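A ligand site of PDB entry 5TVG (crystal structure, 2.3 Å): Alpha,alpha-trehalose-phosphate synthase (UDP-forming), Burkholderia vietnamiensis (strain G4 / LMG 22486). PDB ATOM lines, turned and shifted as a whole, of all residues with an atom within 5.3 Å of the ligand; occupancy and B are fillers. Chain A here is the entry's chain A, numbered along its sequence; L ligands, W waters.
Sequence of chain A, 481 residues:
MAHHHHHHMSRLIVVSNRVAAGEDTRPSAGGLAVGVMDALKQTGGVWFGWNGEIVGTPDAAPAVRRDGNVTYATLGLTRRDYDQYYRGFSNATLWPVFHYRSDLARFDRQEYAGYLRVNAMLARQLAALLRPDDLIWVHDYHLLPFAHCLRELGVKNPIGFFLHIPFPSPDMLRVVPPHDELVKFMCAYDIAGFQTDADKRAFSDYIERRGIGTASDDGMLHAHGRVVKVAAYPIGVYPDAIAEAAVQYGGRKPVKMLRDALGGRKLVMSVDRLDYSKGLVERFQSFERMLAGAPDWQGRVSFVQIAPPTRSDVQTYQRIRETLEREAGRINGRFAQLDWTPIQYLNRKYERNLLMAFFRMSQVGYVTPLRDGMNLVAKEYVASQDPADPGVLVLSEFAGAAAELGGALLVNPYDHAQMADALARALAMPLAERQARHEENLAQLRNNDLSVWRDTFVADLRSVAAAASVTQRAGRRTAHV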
ATOM      1  N   GLY A  30      -3.738  10.007 -31.353  1.00  0.00           N
ATOM      2  CA  GLY A  30      -3.129   9.595 -30.098  1.00  0.00           C
ATOM      3  C   GLY A  30      -2.211   8.410 -30.263  1.00  0.00           C
ATOM      4  O   GLY A  30      -1.242   8.453 -31.044  1.00  0.00           O
ATOM      5  N   GLY A  31      -2.553   7.341 -29.559  1.00  0.00           N
ATOM      6  CA  GLY A  31      -1.940   6.060 -29.766  1.00  0.00           C
ATOM      7  C   GLY A  31      -0.556   5.965 -29.161  1.00  0.00           C
ATOM      8  O   GLY A  31      -0.087   6.831 -28.425  1.00  0.00           O
ATOM      9  N   TRP A  95      -7.247 -11.770 -25.916  1.00  0.00           N
ATOM     10  CA  TRP A  95      -8.085 -10.608 -25.633  1.00  0.00           C
ATOM     11  C   TRP A  95      -9.320 -10.966 -24.802  1.00  0.00           C
ATOM     12  O   TRP A  95      -9.558 -10.295 -23.779  1.00  0.00           O
ATOM     13  CB  TRP A  95      -8.468  -9.890 -26.938  1.00  0.00           C
ATOM     14  CG  TRP A  95      -9.371  -8.712 -26.662  1.00  0.00           C
ATOM     15  CD1 TRP A  95     -10.747  -8.730 -26.544  1.00  0.00           C
ATOM     16  CD2 TRP A  95      -8.982  -7.337 -26.447  1.00  0.00           C
ATOM     17  NE1 TRP A  95     -11.224  -7.468 -26.296  1.00  0.00           N
ATOM     18  CE2 TRP A  95     -10.166  -6.604 -26.217  1.00  0.00           C
ATOM     19  CE3 TRP A  95      -7.758  -6.674 -26.439  1.00  0.00           C
ATOM     20  CZ2 TRP A  95     -10.153  -5.222 -25.968  1.00  0.00           C
ATOM     21  CZ3 TRP A  95      -7.747  -5.313 -26.213  1.00  0.00           C
ATOM     22  CH2 TRP A  95      -8.938  -4.604 -25.982  1.00  0.00           C
ATOM     23  N   VAL A 271     -17.511   7.643 -26.062  1.00  0.00           N
ATOM     24  CA  VAL A 271     -16.673   7.283 -27.220  1.00  0.00           C
ATOM     25  C   VAL A 271     -15.989   5.961 -26.889  1.00  0.00           C
ATOM     26  O   VAL A 271     -15.278   5.859 -25.875  1.00  0.00           O
ATOM     27  CB  VAL A 271     -15.612   8.351 -27.563  1.00  0.00           C
ATOM     28  CG1 VAL A 271     -14.715   7.816 -28.696  1.00  0.00           C
ATOM     29  CG2 VAL A 271     -16.258   9.668 -28.008  1.00  0.00           C
ATOM     30  N   ASP A 272     -16.222   4.941 -27.727  1.00  0.00           N
ATOM     31  CA  ASP A 272     -15.691   3.599 -27.496  1.00  0.00           C
ATOM     32  C   ASP A 272     -15.513   2.881 -28.820  1.00  0.00           C
ATOM     33  O   ASP A 272     -16.400   2.945 -29.668  1.00  0.00           O
ATOM     34  CB  ASP A 272     -16.633   2.727 -26.629  1.00  0.00           C
ATOM     35  CG  ASP A 272     -17.017   3.366 -25.303  1.00  0.00           C
ATOM     36  OD1 ASP A 272     -17.731   4.388 -25.297  1.00  0.00           O
ATOM     37  OD2 ASP A 272     -16.638   2.811 -24.245  1.00  0.00           O
ATOM     38  N   ARG A 273     -14.424   2.123 -28.980  1.00  0.00           N
ATOM     39  CA  ARG A 273     -14.447   1.070 -30.014  1.00  0.00           C
ATOM     40  C   ARG A 273     -15.615   0.119 -29.706  1.00  0.00           C
ATOM     41  O   ARG A 273     -16.021  -0.057 -28.558  1.00  0.00           O
ATOM     42  CB  ARG A 273     -13.145   0.266 -30.077  1.00  0.00           C
ATOM     43  CG  ARG A 273     -11.883   0.993 -30.611  1.00  0.00           C
ATOM     44  CD  ARG A 273     -10.611   0.061 -30.513  1.00  0.00           C
ATOM     45  NE  ARG A 273     -10.403  -0.377 -29.127  1.00  0.00           N
ATOM     46  CZ  ARG A 273     -10.643  -1.614 -28.675  1.00  0.00           C
ATOM     47  NH1 ARG A 273     -11.068  -2.576 -29.508  1.00  0.00           N
ATOM     48  NH2 ARG A 273     -10.484  -1.898 -27.371  1.00  0.00           N
ATOM     49  N   LYS A 278     -16.318  -3.032 -23.639  1.00  0.00           N
ATOM     50  CA  LYS A 278     -16.726  -1.658 -23.341  1.00  0.00           C
ATOM     51  C   LYS A 278     -18.104  -1.571 -22.695  1.00  0.00           C
ATOM     52  O   LYS A 278     -18.510  -0.498 -22.242  1.00  0.00           O
ATOM     53  CB  LYS A 278     -16.634  -0.809 -24.614  1.00  0.00           C
ATOM     54  CG  LYS A 278     -15.192  -0.758 -25.254  1.00  0.00           C
ATOM     55  CD  LYS A 278     -14.136  -0.002 -24.354  1.00  0.00           C
ATOM     56  CE  LYS A 278     -12.720  -0.064 -24.906  1.00  0.00           C
ATOM     57  NZ  LYS A 278     -11.635   0.770 -24.156  1.00  0.00           N
ATOM     58  N   ILE A 306     -20.575   7.489 -29.912  1.00  0.00           N
ATOM     59  CA  ILE A 306     -19.691   7.282 -31.045  1.00  0.00           C
ATOM     60  C   ILE A 306     -18.986   5.961 -30.807  1.00  0.00           C
ATOM     61  O   ILE A 306     -18.341   5.777 -29.768  1.00  0.00           O
ATOM     62  CB  ILE A 306     -18.687   8.436 -31.174  1.00  0.00           C
ATOM     63  CG1 ILE A 306     -19.439   9.722 -31.555  1.00  0.00           C
ATOM     64  CG2 ILE A 306     -17.561   8.077 -32.190  1.00  0.00           C
ATOM     65  CD1 ILE A 306     -18.616  10.955 -31.469  1.00  0.00           C
ATOM     66  N   PRO A 308     -17.006   3.457 -33.343  1.00  0.00           N
ATOM     67  CA  PRO A 308     -16.480   2.929 -34.608  1.00  0.00           C
ATOM     68  C   PRO A 308     -16.245   1.443 -34.542  1.00  0.00           C
ATOM     69  O   PRO A 308     -15.878   0.909 -33.481  1.00  0.00           O
ATOM     70  CB  PRO A 308     -15.148   3.701 -34.797  1.00  0.00           C
ATOM     71  CG  PRO A 308     -14.783   4.184 -33.401  1.00  0.00           C
ATOM     72  CD  PRO A 308     -16.077   4.400 -32.671  1.00  0.00           C
ATOM     73  N   ARG A 348     -19.440   6.206 -37.150  1.00  0.00           N
ATOM     74  CA  ARG A 348     -18.339   6.850 -37.854  1.00  0.00           C
ATOM     75  C   ARG A 348     -17.223   7.209 -36.876  1.00  0.00           C
ATOM     76  O   ARG A 348     -17.434   7.364 -35.674  1.00  0.00           O
ATOM     77  CB  ARG A 348     -18.804   8.081 -38.610  1.00  0.00           C
ATOM     78  CG  ARG A 348     -19.525   9.073 -37.806  1.00  0.00           C
ATOM     79  CD  ARG A 348     -19.915  10.227 -38.684  1.00  0.00           C
ATOM     80  NE  ARG A 348     -20.591   9.765 -39.886  1.00  0.00           N
ATOM     81  CZ  ARG A 348     -21.233  10.575 -40.715  1.00  0.00           C
ATOM     82  NH1 ARG A 348     -21.262  11.880 -40.469  1.00  0.00           N
ATOM     83  NH2 ARG A 348     -21.827  10.081 -41.794  1.00  0.00           N
ATOM     84  N   LYS A 349     -16.017   7.347 -37.417  1.00  0.00           N
ATOM     85  CA  LYS A 349     -14.847   7.767 -36.674  1.00  0.00           C
ATOM     86  C   LYS A 349     -14.674   9.278 -36.794  1.00  0.00           C
ATOM     87  O   LYS A 349     -15.060   9.870 -37.812  1.00  0.00           O
ATOM     88  CB  LYS A 349     -13.606   7.050 -37.197  1.00  0.00           C
ATOM     89  CG  LYS A 349     -12.424   7.027 -36.249  1.00  0.00           C
ATOM     90  CD  LYS A 349     -11.122   6.841 -37.016  1.00  0.00           C
ATOM     91  CE  LYS A 349     -10.230   5.808 -36.360  1.00  0.00           C
ATOM     92  NZ  LYS A 349      -9.648   6.275 -35.068  1.00  0.00           N
ATOM     93  N   TYR A 350     -14.235   9.912 -35.719  1.00  0.00           N
ATOM     94  CA  TYR A 350     -13.985  11.355 -35.722  1.00  0.00           C
ATOM     95  C   TYR A 350     -12.540  11.638 -35.360  1.00  0.00           C
ATOM     96  O   TYR A 350     -11.904  10.892 -34.614  1.00  0.00           O
ATOM     97  CB  TYR A 350     -14.916  12.132 -34.735  1.00  0.00           C
ATOM     98  CG  TYR A 350     -16.365  12.203 -35.175  1.00  0.00           C
ATOM     99  CD1 TYR A 350     -17.226  11.131 -35.006  1.00  0.00           C
ATOM    100  CD2 TYR A 350     -16.857  13.337 -35.829  1.00  0.00           C
ATOM    101  CE1 TYR A 350     -18.577  11.198 -35.427  1.00  0.00           C
ATOM    102  CE2 TYR A 350     -18.192  13.412 -36.267  1.00  0.00           C
ATOM    103  CZ  TYR A 350     -19.045  12.334 -36.063  1.00  0.00           C
ATOM    104  OH  TYR A 350     -20.351  12.413 -36.508  1.00  0.00           O
ATOM    105  N   GLU A 351     -12.045  12.749 -35.908  1.00  0.00           N
ATOM    106  CA  GLU A 351     -10.745  13.276 -35.542  1.00  0.00           C
ATOM    107  C   GLU A 351     -10.675  13.467 -34.025  1.00  0.00           C
ATOM    108  O   GLU A 351     -11.607  14.011 -33.420  1.00  0.00           O
ATOM    109  CB  GLU A 351     -10.546  14.602 -36.270  1.00  0.00           C
ATOM    110  CG  GLU A 351      -9.137  15.156 -36.331  1.00  0.00           C
ATOM    111  CD  GLU A 351      -9.137  16.615 -36.755  1.00  0.00           C
ATOM    112  OE1 GLU A 351     -10.137  17.055 -37.374  1.00  0.00           O
ATOM    113  OE2 GLU A 351      -8.131  17.320 -36.442  1.00  0.00           O
ATOM    114  N   ARG A 352      -9.576  13.018 -33.428  1.00  0.00           N
ATOM    115  CA  ARG A 352      -9.457  12.988 -31.964  1.00  0.00           C
ATOM    116  C   ARG A 352      -9.661  14.375 -31.340  1.00  0.00           C
ATOM    117  O   ARG A 352     -10.271  14.493 -30.278  1.00  0.00           O
ATOM    118  CB  ARG A 352      -8.097  12.414 -31.575  1.00  0.00           C
ATOM    119  CG  ARG A 352      -8.019  11.914 -30.162  1.00  0.00           C
ATOM    120  CD  ARG A 352      -6.848  10.972 -29.923  1.00  0.00           C
ATOM    121  NE  ARG A 352      -6.480  11.015 -28.498  1.00  0.00           N
ATOM    122  CZ  ARG A 352      -5.646  11.920 -28.004  1.00  0.00           C
ATOM    123  NH1 ARG A 352      -5.111  12.805 -28.834  1.00  0.00           N
ATOM    124  NH2 ARG A 352      -5.341  11.934 -26.700  1.00  0.00           N
ATOM    125  N   LEU A 355     -13.258  14.991 -30.882  1.00  0.00           N
ATOM    126  CA  LEU A 355     -13.762  14.287 -29.706  1.00  0.00           C
ATOM    127  C   LEU A 355     -13.606  15.125 -28.433  1.00  0.00           C
ATOM    128  O   LEU A 355     -14.495  15.140 -27.579  1.00  0.00           O
ATOM    129  CB  LEU A 355     -13.056  12.933 -29.575  1.00  0.00           C
ATOM    130  CG  LEU A 355     -13.298  11.886 -30.664  1.00  0.00           C
ATOM    131  CD1 LEU A 355     -12.637  10.593 -30.277  1.00  0.00           C
ATOM    132  CD2 LEU A 355     -14.800  11.652 -30.874  1.00  0.00           C
ATOM    133  N   MET A 356     -12.476  15.836 -28.308  1.00  0.00           N
ATOM    134  CA  MET A 356     -12.257  16.674 -27.123  1.00  0.00           C
ATOM    135  C   MET A 356     -13.271  17.813 -27.044  1.00  0.00           C
ATOM    136  O   MET A 356     -13.767  18.133 -25.957  1.00  0.00           O
ATOM    137  CB  MET A 356     -10.825  17.223 -27.130  1.00  0.00           C
ATOM    138  CG  MET A 356      -9.775  16.108 -27.359  1.00  0.00           C
ATOM    139  SD  MET A 356      -9.953  14.738 -26.184  1.00  0.00           S
ATOM    140  CE  MET A 356      -9.143  13.408 -27.029  1.00  0.00           C
ATOM    141  N   ASP A 372     -11.228  -2.951 -18.557  1.00  0.00           N
ATOM    142  CA  ASP A 372     -10.339  -2.134 -19.369  1.00  0.00           C
ATOM    143  C   ASP A 372      -8.981  -1.985 -18.690  1.00  0.00           C
ATOM    144  O   ASP A 372      -8.913  -1.740 -17.473  1.00  0.00           O
ATOM    145  CB  ASP A 372     -10.950  -0.764 -19.622  1.00  0.00           C
ATOM    146  CG  ASP A 372     -11.043  -0.414 -21.098  1.00  0.00           C
ATOM    147  OD1 ASP A 372     -10.270  -0.987 -21.930  1.00  0.00           O
ATOM    148  OD2 ASP A 372     -11.911   0.422 -21.439  1.00  0.00           O
ATOM    149  N   ASN A 375      -8.237   2.736 -19.933  1.00  0.00           N
ATOM    150  CA  ASN A 375      -9.243   3.604 -20.553  1.00  0.00           C
ATOM    151  C   ASN A 375      -8.813   5.070 -20.518  1.00  0.00           C
ATOM    152  O   ASN A 375      -9.005   5.769 -19.503  1.00  0.00           O
ATOM    153  CB  ASN A 375     -10.645   3.471 -19.917  1.00  0.00           C
ATOM    154  CG  ASN A 375     -11.731   4.102 -20.806  1.00  0.00           C
ATOM    155  OD1 ASN A 375     -11.746   5.323 -21.022  1.00  0.00           O
ATOM    156  ND2 ASN A 375     -12.614   3.254 -21.351  1.00  0.00           N
ATOM    157  N   LEU A 376      -8.256   5.559 -21.629  1.00  0.00           N
ATOM    158  CA  LEU A 376      -7.762   6.939 -21.732  1.00  0.00           C
ATOM    159  C   LEU A 376      -8.874   7.925 -22.056  1.00  0.00           C
ATOM    160  O   LEU A 376      -8.748   9.117 -21.741  1.00  0.00           O
ATOM    161  CB  LEU A 376      -6.666   7.023 -22.806  1.00  0.00           C
ATOM    162  CG  LEU A 376      -5.385   6.258 -22.519  1.00  0.00           C
ATOM    163  CD1 LEU A 376      -4.391   6.345 -23.722  1.00  0.00           C
ATOM    164  CD2 LEU A 376      -4.772   6.793 -21.185  1.00  0.00           C
ATOM    165  N   VAL A 377      -9.948   7.461 -22.718  1.00  0.00           N
ATOM    166  CA  VAL A 377     -11.135   8.298 -22.908  1.00  0.00           C
ATOM    167  C   VAL A 377     -11.576   8.903 -21.580  1.00  0.00           C
ATOM    168  O   VAL A 377     -11.894  10.101 -21.495  1.00  0.00           O
ATOM    169  CB  VAL A 377     -12.263   7.483 -23.561  1.00  0.00           C
ATOM    170  CG1 VAL A 377     -13.651   8.199 -23.423  1.00  0.00           C
ATOM    171  CG2 VAL A 377     -11.942   7.192 -25.053  1.00  0.00           C
ATOM    172  N   GLU A 380      -9.164  11.596 -20.890  1.00  0.00           N
ATOM    173  CA  GLU A 380      -9.359  12.630 -21.901  1.00  0.00           C
ATOM    174  C   GLU A 380     -10.622  13.408 -21.623  1.00  0.00           C
ATOM    175  O   GLU A 380     -10.673  14.632 -21.812  1.00  0.00           O
ATOM    176  CB  GLU A 380      -9.422  12.021 -23.313  1.00  0.00           C
ATOM    177  CG  GLU A 380      -8.076  11.431 -23.798  1.00  0.00           C
ATOM    178  CD  GLU A 380      -8.249  10.548 -25.037  1.00  0.00           C
ATOM    179  OE1 GLU A 380      -7.232  10.094 -25.574  1.00  0.00           O
ATOM    180  OE2 GLU A 380      -9.400  10.273 -25.461  1.00  0.00           O
HETATM  181  N1  LIG L   1     -10.210   7.405 -30.208  1.00  0.00           N
HETATM  182  C1  LIG L   1     -10.209   8.289 -31.261  1.00  0.00           C
HETATM  183  N2  LIG L   1     -11.283   8.214 -32.105  1.00  0.00           N
HETATM  184  C2  LIG L   1     -12.351   7.331 -32.009  1.00  0.00           C
HETATM  185  C3  LIG L   1     -12.283   6.436 -30.884  1.00  0.00           C
HETATM  186  C4  LIG L   1     -11.228   6.483 -30.046  1.00  0.00           C
HETATM  187  O1  LIG L   1      -9.327   9.120 -31.438  1.00  0.00           O
HETATM  188  O2  LIG L   1     -13.249   7.373 -32.878  1.00  0.00           O
HETATM  189  C5  LIG L   1      -9.063   7.456 -29.276  1.00  0.00           C
HETATM  190  C6  LIG L   1      -9.334   8.045 -27.891  1.00  0.00           C
HETATM  191  O3  LIG L   1      -9.091   9.442 -27.950  1.00  0.00           O
HETATM  192  C7  LIG L   1      -8.237   7.380 -27.065  1.00  0.00           C
HETATM  193  C8  LIG L   1      -8.140   5.995 -27.707  1.00  0.00           C
HETATM  194  O4  LIG L   1      -8.592   6.149 -29.061  1.00  0.00           O
HETATM  195  O5  LIG L   1      -6.985   8.060 -27.058  1.00  0.00           O
HETATM  196  C9  LIG L   1      -9.057   5.005 -27.034  1.00  0.00           C
HETATM  197  O6  LIG L   1      -8.203   4.360 -26.080  1.00  0.00           O
HETATM  198  P1  LIG L   1      -8.763   3.799 -24.737  1.00  0.00           P
HETATM  199  O7  LIG L   1      -7.581   3.595 -23.853  1.00  0.00           O
HETATM  200  O8  LIG L   1      -9.906   4.653 -24.202  1.00  0.00           O
HETATM  201  O9  LIG L   1      -9.382   2.387 -25.131  1.00  0.00           O
HETATM  202  P2  LIG L   1      -8.882   1.405 -26.279  1.00  0.00           P
HETATM  203  O10 LIG L   1      -7.355   1.537 -26.251  1.00  0.00           O
HETATM  204  O11 LIG L   1      -9.137   0.017 -25.703  1.00  0.00           O
HETATM  205  O12 LIG L   1      -9.556   1.686 -27.577  1.00  0.00           O
HETATM  206  O   HOH W   1      -8.667   2.873 -29.624  1.00  0.00           O
HETATM  207  O   HOH W   2      -6.266  -0.906 -27.821  1.00  0.00           O
HETATM  208  O   HOH W   3      -5.917   6.464 -30.844  1.00  0.00           O
HETATM  209  O   HOH W   4      -5.209   2.642 -25.579  1.00  0.00           O
HETATM  210  O   HOH W   5     -12.046   2.686 -27.300  1.00  0.00           O
HETATM  211  O   HOH W   6     -12.197   3.351 -24.708  1.00  0.00           O
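O5 of the ligand is in hydrogen-bond range of OE1 of Glu 380.
An oxygen (O12) of the ligand lies within salt-bridge range of the guanidinium group (NE) of Arg 273 (2.7 Å).
An oxygen (O11) of the ligand is in salt-bridge range of the side-chain amino group (NZ) of Lys 278 (3.0 Å).
O7 of the ligand sits at hydrogen-bond distance from N of Leu 376, at 3.0 Å.
The guanidinium group of Arg 352 is in hydrogen-bond range of an oxygen (O3) of the ligand (3.1 Å).
O8 of the ligand sits at hydrogen-bond distance from N of Val 377 (3.2 Å).
The side-chain carboxylate (OE1) of Glu 380 is in salt-bridge range of the guanidinium group (NH2) of Arg 352 (2.9 Å).
NZ of Lys 278 lies within salt-bridge range of OD2 of Asp 372 (2.8 Å).
The backbone NH (N) of Val 377 lies within hydrogen-bond range of the side-chain amide oxygen (OD1) of Asn 375 (3.3 Å).
The side-chain amide nitrogen (ND2) of Asn 375 is in hydrogen-bond range of the side-chain carboxylate (OD2) of Asp 372, 2.9 Å away.
Merely in contact with the ligand: Leu 355, Lys 349, Val 271, Pro 308, Asn 375 and Tyr 350.
Hydrophobic or aromatic side chains within 4 Å of the ligand: Val 271, Pro 308, Leu 355, Leu 376 and Val 377.
12 residues have an atom within 4 Å of the ligand: Val 271, Arg 273, Lys 278, Pro 308, Lys 349, Tyr 350, Arg 352, Leu 355, Asn 375, Leu 376, Val 377 and Glu 380.
Water W6 lies within hydrogen-bond range of an oxygen (O8) of the ligand (2.7 Å), the side-chain amino group (NZ) of Lys 278 (2.7 Å) and the side-chain amide nitrogen (ND2) of Asn 375 (3.4 Å).
Water W5 bridges an oxygen (O12) of the ligand (2.7 Å) and the backbone NH (N) of Arg 273 (3.0 Å).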
